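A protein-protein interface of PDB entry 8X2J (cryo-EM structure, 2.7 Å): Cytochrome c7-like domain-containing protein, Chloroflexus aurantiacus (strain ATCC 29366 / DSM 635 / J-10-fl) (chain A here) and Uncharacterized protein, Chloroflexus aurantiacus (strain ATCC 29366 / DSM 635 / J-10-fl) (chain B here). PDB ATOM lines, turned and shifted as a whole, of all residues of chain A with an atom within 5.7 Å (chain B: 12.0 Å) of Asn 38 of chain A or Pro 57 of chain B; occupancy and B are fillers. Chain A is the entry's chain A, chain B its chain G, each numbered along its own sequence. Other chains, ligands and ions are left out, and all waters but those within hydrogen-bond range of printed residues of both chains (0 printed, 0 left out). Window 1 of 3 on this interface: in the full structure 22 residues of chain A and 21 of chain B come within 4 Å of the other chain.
N of Asn 38 of chain A sits at hydrogen-bond distance from O of Gly 54 of chain B (3.1 Å). ND2 of Asn 38 of chain A lies within hydrogen-bond range of O of Pro 57 of chain B, at 3.0 Å. The side-chain amide nitrogen (ND2) of Asn 44 of chain A sits at hydrogen-bond distance from the side-chain hydroxyl (OG1) of Thr 59 of chain B (3.2 Å). O of Phe 58 of chain B lies close to O of Asn 44 of chain A (3.4 Å).
The side-chain hydroxyl of Ser 37 of chain A sits close to the backbone NH of Phe 40 of chain A, at 3.5 Å. O of Asn 38 of chain A is in hydrogen-bond range of N of Val 43 of chain A (2.8 Å). The side-chain amide oxygen of Asn 44 of chain A is in hydrogen-bond range of the side-chain amide nitrogen of Asn 38 of chain A, 3.4 Å away. The backbone carbonyl oxygen (O) of Thr 59 of chain B sits at hydrogen-bond distance from the side-chain amide nitrogen (NE2) of Gln 61 of chain B, 2.9 Å away.
Of the 10 printed residues of chain A, 4 touch a printed residue of chain B. Along chain A the printed residues that touch a printed residue of chain B span positions 37 to 44. Among the printed residues, 8 pairs touch across the chains. Among the printed residues, no Asp or Glu carboxylate lies within 4 Å of a Lys or Arg side-chain nitrogen of the other chain.
Among the printed residues, pairs that only touch across the chains: Ser 37 of chain A with Gly 54 of chain B (3.5 Å), Asn 44 of chain A with Pro 57 of chain B (3.5 Å), Asn 44 of chain A with Pro 60 of chain B (3.8 Å) and Val 43 of chain A with Pro 57 of chain B (3.9 Å).
Pro 57 of chain B touches just these residues of chain A: Asn 38, Val 43 and Asn 44. No residue of chain B comes within 4 Å of Gln 42 of chain A. Of chain B, only Pro 57 (3.9 Å) comes within 4 Å of Val 43 of chain A. Of the printed residues of chain A, Gly 54 of chain B touches Ser 37 (3.5 Å) and Asn 38 (3.1 Å). Of the printed residues of chain A, Thr 59 of chain B touches Asn 44. Leu 48 of chain B touches none of the printed residues of chain A. The nearest residue of chain A that does not touch Pro 57 of chain B is Tyr 39 of chain A (4.2 Å). The nearest printed residue of chain A that does not touch Gly 54 of chain B is Tyr 39 of chain A (4.9 Å).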
ATOM      1  N   ARG A  36       5.616  23.244  -7.100  1.00  0.00           N
ATOM      2  CA  ARG A  36       5.582  22.475  -8.336  1.00  0.00           C
ATOM      3  C   ARG A  36       4.320  22.698  -9.161  1.00  0.00           C
ATOM      4  O   ARG A  36       4.167  22.065 -10.210  1.00  0.00           O
ATOM      5  CB  ARG A  36       5.730  20.983  -8.024  1.00  0.00           C
ATOM      6  CG  ARG A  36       7.124  20.585  -7.594  1.00  0.00           C
ATOM      7  CD  ARG A  36       7.086  19.432  -6.616  1.00  0.00           C
ATOM      8  NE  ARG A  36       8.355  18.721  -6.542  1.00  0.00           N
ATOM      9  CZ  ARG A  36       9.372  19.084  -5.773  1.00  0.00           C
ATOM     10  NH1 ARG A  36       9.313  20.165  -5.014  1.00  0.00           N
ATOM     11  NH2 ARG A  36      10.477  18.344  -5.768  1.00  0.00           N
ATOM     12  N   SER A  37       3.413  23.566  -8.717  1.00  0.00           N
ATOM     13  CA  SER A  37       2.113  23.710  -9.355  1.00  0.00           C
ATOM     14  C   SER A  37       2.193  24.433 -10.696  1.00  0.00           C
ATOM     15  O   SER A  37       3.104  25.223 -10.972  1.00  0.00           O
ATOM     16  CB  SER A  37       1.150  24.453  -8.430  1.00  0.00           C
ATOM     17  OG  SER A  37       1.671  25.713  -8.055  1.00  0.00           O
ATOM     18  N   ASN A  38       1.189  24.149 -11.533  1.00  0.00           N
ATOM     19  CA  ASN A  38       1.091  24.748 -12.858  1.00  0.00           C
ATOM     20  C   ASN A  38       0.786  26.236 -12.790  1.00  0.00           C
ATOM     21  O   ASN A  38       1.160  26.978 -13.701  1.00  0.00           O
ATOM     22  CB  ASN A  38       0.015  24.034 -13.674  1.00  0.00           C
ATOM     23  CG  ASN A  38       0.423  22.639 -14.082  1.00  0.00           C
ATOM     24  OD1 ASN A  38       1.514  22.180 -13.754  1.00  0.00           O
ATOM     25  ND2 ASN A  38      -0.455  21.954 -14.801  1.00  0.00           N
ATOM     26  N   TYR A  39       0.099  26.691 -11.739  1.00  0.00           N
ATOM     27  CA  TYR A  39      -0.130  28.122 -11.573  1.00  0.00           C
ATOM     28  C   TYR A  39       1.169  28.851 -11.253  1.00  0.00           C
ATOM     29  O   TYR A  39       1.435  29.928 -11.799  1.00  0.00           O
ATOM     30  CB  TYR A  39      -1.164  28.371 -10.474  1.00  0.00           C
ATOM     31  CG  TYR A  39      -1.099  29.765  -9.888  1.00  0.00           C
ATOM     32  CD1 TYR A  39      -1.545  30.862 -10.617  1.00  0.00           C
ATOM     33  CD2 TYR A  39      -0.585  29.987  -8.615  1.00  0.00           C
ATOM     34  CE1 TYR A  39      -1.482  32.138 -10.096  1.00  0.00           C
ATOM     35  CE2 TYR A  39      -0.513  31.261  -8.090  1.00  0.00           C
ATOM     36  CZ  TYR A  39      -0.966  32.331  -8.833  1.00  0.00           C
ATOM     37  OH  TYR A  39      -0.903  33.601  -8.312  1.00  0.00           O
ATOM     38  N   PHE A  40       1.971  28.288 -10.349  1.00  0.00           N
ATOM     39  CA  PHE A  40       3.241  28.895  -9.971  1.00  0.00           C
ATOM     40  C   PHE A  40       4.229  28.873 -11.126  1.00  0.00           C
ATOM     41  O   PHE A  40       4.943  29.855 -11.357  1.00  0.00           O
ATOM     42  CB  PHE A  40       3.809  28.165  -8.758  1.00  0.00           C
ATOM     43  CG  PHE A  40       5.086  28.744  -8.222  1.00  0.00           C
ATOM     44  CD1 PHE A  40       5.086  29.946  -7.537  1.00  0.00           C
ATOM     45  CD2 PHE A  40       6.281  28.061  -8.364  1.00  0.00           C
ATOM     46  CE1 PHE A  40       6.262  30.469  -7.026  1.00  0.00           C
ATOM     47  CE2 PHE A  40       7.459  28.577  -7.857  1.00  0.00           C
ATOM     48  CZ  PHE A  40       7.447  29.782  -7.187  1.00  0.00           C
ATOM     49  N   ARG A  41       4.269  27.777 -11.875  1.00  0.00           N
ATOM     50  CA  ARG A  41       5.223  27.646 -12.964  1.00  0.00           C
ATOM     51  C   ARG A  41       4.667  28.103 -14.308  1.00  0.00           C
ATOM     52  O   ARG A  41       5.382  28.002 -15.312  1.00  0.00           O
ATOM     53  CB  ARG A  41       5.702  26.196 -13.055  1.00  0.00           C
ATOM     54  CG  ARG A  41       6.382  25.688 -11.796  1.00  0.00           C
ATOM     55  CD  ARG A  41       7.575  26.543 -11.434  1.00  0.00           C
ATOM     56  NE  ARG A  41       8.475  26.720 -12.566  1.00  0.00           N
ATOM     57  CZ  ARG A  41       9.777  26.484 -12.533  1.00  0.00           C
ATOM     58  NH1 ARG A  41      10.375  26.065 -11.431  1.00  0.00           N
ATOM     59  NH2 ARG A  41      10.498  26.680 -13.631  1.00  0.00           N
ATOM     60  N   GLN A  42       3.425  28.608 -14.329  1.00  0.00           N
ATOM     61  CA  GLN A  42       2.736  29.123 -15.521  1.00  0.00           C
ATOM     62  C   GLN A  42       2.639  28.072 -16.630  1.00  0.00           C
ATOM     63  O   GLN A  42       2.871  28.349 -17.807  1.00  0.00           O
ATOM     64  CB  GLN A  42       3.389  30.413 -16.026  1.00  0.00           C
ATOM     65  CG  GLN A  42       3.148  31.612 -15.122  1.00  0.00           C
ATOM     66  CD  GLN A  42       1.676  31.883 -14.897  1.00  0.00           C
ATOM     67  OE1 GLN A  42       0.974  32.336 -15.798  1.00  0.00           O
ATOM     68  NE2 GLN A  42       1.201  31.604 -13.690  1.00  0.00           N
ATOM     69  N   VAL A  43       2.263  26.858 -16.239  1.00  0.00           N
ATOM     70  CA  VAL A  43       2.174  25.712 -17.138  1.00  0.00           C
ATOM     71  C   VAL A  43       0.710  25.469 -17.477  1.00  0.00           C
ATOM     72  O   VAL A  43      -0.166  25.625 -16.618  1.00  0.00           O
ATOM     73  CB  VAL A  43       2.825  24.472 -16.491  1.00  0.00           C
ATOM     74  CG1 VAL A  43       2.790  23.261 -17.405  1.00  0.00           C
ATOM     75  CG2 VAL A  43       4.247  24.783 -16.124  1.00  0.00           C
ATOM     76  N   ASN A  44       0.448  25.149 -18.753  1.00  0.00           N
ATOM     77  CA  ASN A  44      -0.870  24.772 -19.282  1.00  0.00           C
ATOM     78  C   ASN A  44      -1.889  25.901 -19.161  1.00  0.00           C
ATOM     79  O   ASN A  44      -3.094  25.657 -19.083  1.00  0.00           O
ATOM     80  CB  ASN A  44      -1.408  23.494 -18.627  1.00  0.00           C
ATOM     81  CG  ASN A  44      -0.597  22.269 -18.985  1.00  0.00           C
ATOM     82  OD1 ASN A  44      -0.073  21.584 -18.112  1.00  0.00           O
ATOM     83  ND2 ASN A  44      -0.489  21.988 -20.276  1.00  0.00           N
ATOM     84  N   VAL A  45      -1.416  27.143 -19.162  1.00  0.00           N
ATOM     85  CA  VAL A  45      -2.277  28.318 -19.149  1.00  0.00           C
ATOM     86  C   VAL A  45      -1.994  29.128 -20.411  1.00  0.00           C
ATOM     87  O   VAL A  45      -0.833  29.359 -20.769  1.00  0.00           O
ATOM     88  CB  VAL A  45      -2.102  29.145 -17.853  1.00  0.00           C
ATOM     89  CG1 VAL A  45      -0.648  29.515 -17.580  1.00  0.00           C
ATOM     90  CG2 VAL A  45      -2.972  30.394 -17.884  1.00  0.00           C
ATOM     91  N   LEU B  48      -5.034  14.827  -1.443  1.00  0.00           N
ATOM     92  CA  LEU B  48      -5.392  14.635  -2.848  1.00  0.00           C
ATOM     93  C   LEU B  48      -6.069  15.864  -3.446  1.00  0.00           C
ATOM     94  O   LEU B  48      -5.857  16.159  -4.629  1.00  0.00           O
ATOM     95  CB  LEU B  48      -6.271  13.394  -3.021  1.00  0.00           C
ATOM     96  CG  LEU B  48      -5.565  12.068  -3.339  1.00  0.00           C
ATOM     97  CD1 LEU B  48      -4.737  11.511  -2.203  1.00  0.00           C
ATOM     98  CD2 LEU B  48      -6.597  11.045  -3.782  1.00  0.00           C
ATOM     99  N   VAL B  49      -6.853  16.602  -2.651  1.00  0.00           N
ATOM    100  CA  VAL B  49      -7.391  17.882  -3.119  1.00  0.00           C
ATOM    101  C   VAL B  49      -6.264  18.883  -3.371  1.00  0.00           C
ATOM    102  O   VAL B  49      -6.285  19.623  -4.365  1.00  0.00           O
ATOM    103  CB  VAL B  49      -8.441  18.419  -2.124  1.00  0.00           C
ATOM    104  CG1 VAL B  49      -8.905  19.816  -2.502  1.00  0.00           C
ATOM    105  CG2 VAL B  49      -9.652  17.510  -2.119  1.00  0.00           C
ATOM    106  N   VAL B  50      -5.245  18.890  -2.505  1.00  0.00           N
ATOM    107  CA  VAL B  50      -4.098  19.784  -2.687  1.00  0.00           C
ATOM    108  C   VAL B  50      -3.312  19.424  -3.950  1.00  0.00           C
ATOM    109  O   VAL B  50      -2.947  20.307  -4.736  1.00  0.00           O
ATOM    110  CB  VAL B  50      -3.215  19.766  -1.423  1.00  0.00           C
ATOM    111  CG1 VAL B  50      -1.806  20.258  -1.711  1.00  0.00           C
ATOM    112  CG2 VAL B  50      -3.844  20.617  -0.334  1.00  0.00           C
ATOM    113  N   LEU B  51      -3.077  18.126  -4.185  1.00  0.00           N
ATOM    114  CA  LEU B  51      -2.377  17.675  -5.392  1.00  0.00           C
ATOM    115  C   LEU B  51      -3.162  18.005  -6.662  1.00  0.00           C
ATOM    116  O   LEU B  51      -2.581  18.447  -7.666  1.00  0.00           O
ATOM    117  CB  LEU B  51      -2.107  16.167  -5.315  1.00  0.00           C
ATOM    118  CG  LEU B  51      -0.826  15.529  -4.740  1.00  0.00           C
ATOM    119  CD1 LEU B  51       0.378  15.822  -5.588  1.00  0.00           C
ATOM    120  CD2 LEU B  51      -0.529  15.944  -3.326  1.00  0.00           C
ATOM    121  N   LEU B  52      -4.487  17.813  -6.632  1.00  0.00           N
ATOM    122  CA  LEU B  52      -5.311  18.141  -7.790  1.00  0.00           C
ATOM    123  C   LEU B  52      -5.368  19.645  -8.030  1.00  0.00           C
ATOM    124  O   LEU B  52      -5.451  20.079  -9.182  1.00  0.00           O
ATOM    125  CB  LEU B  52      -6.715  17.554  -7.609  1.00  0.00           C
ATOM    126  CG  LEU B  52      -7.747  17.524  -8.745  1.00  0.00           C
ATOM    127  CD1 LEU B  52      -8.632  16.308  -8.564  1.00  0.00           C
ATOM    128  CD2 LEU B  52      -8.627  18.766  -8.790  1.00  0.00           C
ATOM    129  N   ALA B  53      -5.327  20.453  -6.967  1.00  0.00           N
ATOM    130  CA  ALA B  53      -5.262  21.900  -7.142  1.00  0.00           C
ATOM    131  C   ALA B  53      -3.890  22.340  -7.628  1.00  0.00           C
ATOM    132  O   ALA B  53      -3.757  23.412  -8.228  1.00  0.00           O
ATOM    133  CB  ALA B  53      -5.612  22.607  -5.835  1.00  0.00           C
ATOM    134  N   GLY B  54      -2.856  21.554  -7.341  1.00  0.00           N
ATOM    135  CA  GLY B  54      -1.559  21.805  -7.946  1.00  0.00           C
ATOM    136  C   GLY B  54      -1.551  21.511  -9.433  1.00  0.00           C
ATOM    137  O   GLY B  54      -0.869  22.189 -10.205  1.00  0.00           O
ATOM    138  N   ARG B  55      -2.294  20.488  -9.854  1.00  0.00           N
ATOM    139  CA  ARG B  55      -2.466  20.191 -11.273  1.00  0.00           C
ATOM    140  C   ARG B  55      -3.758  20.774 -11.838  1.00  0.00           C
ATOM    141  O   ARG B  55      -4.264  20.274 -12.848  1.00  0.00           O
ATOM    142  CB  ARG B  55      -2.432  18.682 -11.511  1.00  0.00           C
ATOM    143  CG  ARG B  55      -1.101  18.021 -11.229  1.00  0.00           C
ATOM    144  CD  ARG B  55      -0.032  18.457 -12.214  1.00  0.00           C
ATOM    145  NE  ARG B  55      -0.370  18.086 -13.583  1.00  0.00           N
ATOM    146  CZ  ARG B  55      -0.081  16.918 -14.140  1.00  0.00           C
ATOM    147  NH1 ARG B  55       0.557  15.972 -13.470  1.00  0.00           N
ATOM    148  NH2 ARG B  55      -0.441  16.694 -15.400  1.00  0.00           N
ATOM    149  N   LEU B  56      -4.311  21.815 -11.201  1.00  0.00           N
ATOM    150  CA  LEU B  56      -5.613  22.384 -11.558  1.00  0.00           C
ATOM    151  C   LEU B  56      -5.685  22.986 -12.964  1.00  0.00           C
ATOM    152  O   LEU B  56      -6.701  22.770 -13.637  1.00  0.00           O
ATOM    153  CB  LEU B  56      -6.062  23.417 -10.519  1.00  0.00           C
ATOM    154  CG  LEU B  56      -7.570  23.646 -10.436  1.00  0.00           C
ATOM    155  CD1 LEU B  56      -8.293  22.341 -10.132  1.00  0.00           C
ATOM    156  CD2 LEU B  56      -7.895  24.705  -9.393  1.00  0.00           C
ATOM    157  N   PRO B  57      -4.675  23.757 -13.476  1.00  0.00           N
ATOM    158  CA  PRO B  57      -4.722  24.057 -14.913  1.00  0.00           C
ATOM    159  C   PRO B  57      -4.363  22.828 -15.729  1.00  0.00           C
ATOM    160  O   PRO B  57      -3.190  22.460 -15.827  1.00  0.00           O
ATOM    161  CB  PRO B  57      -3.688  25.178 -15.087  1.00  0.00           C
ATOM    162  CG  PRO B  57      -3.459  25.707 -13.730  1.00  0.00           C
ATOM    163  CD  PRO B  57      -3.588  24.527 -12.838  1.00  0.00           C
ATOM    164  N   PHE B  58      -5.369  22.187 -16.314  1.00  0.00           N
ATOM    165  CA  PHE B  58      -5.134  21.006 -17.123  1.00  0.00           C
ATOM    166  C   PHE B  58      -4.589  21.409 -18.489  1.00  0.00           C
ATOM    167  O   PHE B  58      -4.588  22.586 -18.862  1.00  0.00           O
ATOM    168  CB  PHE B  58      -6.419  20.196 -17.281  1.00  0.00           C
ATOM    169  CG  PHE B  58      -6.799  19.414 -16.058  1.00  0.00           C
ATOM    170  CD1 PHE B  58      -5.832  18.774 -15.298  1.00  0.00           C
ATOM    171  CD2 PHE B  58      -8.127  19.314 -15.671  1.00  0.00           C
ATOM    172  CE1 PHE B  58      -6.183  18.050 -14.170  1.00  0.00           C
ATOM    173  CE2 PHE B  58      -8.484  18.593 -14.545  1.00  0.00           C
ATOM    174  CZ  PHE B  58      -7.510  17.960 -13.794  1.00  0.00           C
ATOM    175  N   THR B  59      -4.115  20.418 -19.232  1.00  0.00           N
ATOM    176  CA  THR B  59      -3.635  20.659 -20.588  1.00  0.00           C
ATOM    177  C   THR B  59      -4.816  21.023 -21.474  1.00  0.00           C
ATOM    178  O   THR B  59      -5.802  20.274 -21.508  1.00  0.00           O
ATOM    179  CB  THR B  59      -2.913  19.430 -21.131  1.00  0.00           C
ATOM    180  OG1 THR B  59      -1.866  19.053 -20.230  1.00  0.00           O
ATOM    181  CG2 THR B  59      -2.309  19.725 -22.495  1.00  0.00           C
ATOM    182  N   PRO B  60      -4.786  22.167 -22.160  1.00  0.00           N
ATOM    183  CA  PRO B  60      -5.951  22.598 -22.940  1.00  0.00           C
ATOM    184  C   PRO B  60      -6.210  21.709 -24.144  1.00  0.00           C
ATOM    185  O   PRO B  60      -5.297  21.109 -24.716  1.00  0.00           O
ATOM    186  CB  PRO B  60      -5.581  24.022 -23.373  1.00  0.00           C
ATOM    187  CG  PRO B  60      -4.504  24.446 -22.433  1.00  0.00           C
ATOM    188  CD  PRO B  60      -3.745  23.204 -22.111  1.00  0.00           C
ATOM    189  N   GLN B  61      -7.486  21.624 -24.515  1.00  0.00           N
ATOM    190  CA  GLN B  61      -7.948  20.812 -25.639  1.00  0.00           C
ATOM    191  C   GLN B  61      -8.500  21.760 -26.693  1.00  0.00           C
ATOM    192  O   GLN B  61      -9.667  22.174 -26.618  1.00  0.00           O
ATOM    193  CB  GLN B  61      -9.006  19.802 -25.198  1.00  0.00           C
ATOM    194  CG  GLN B  61      -8.611  18.968 -23.993  1.00  0.00           C
ATOM    195  CD  GLN B  61      -7.428  18.066 -24.275  1.00  0.00           C
ATOM    196  OE1 GLN B  61      -7.500  17.176 -25.123  1.00  0.00           O
ATOM    197  NE2 GLN B  61      -6.330  18.287 -23.561  1.00  0.00           N
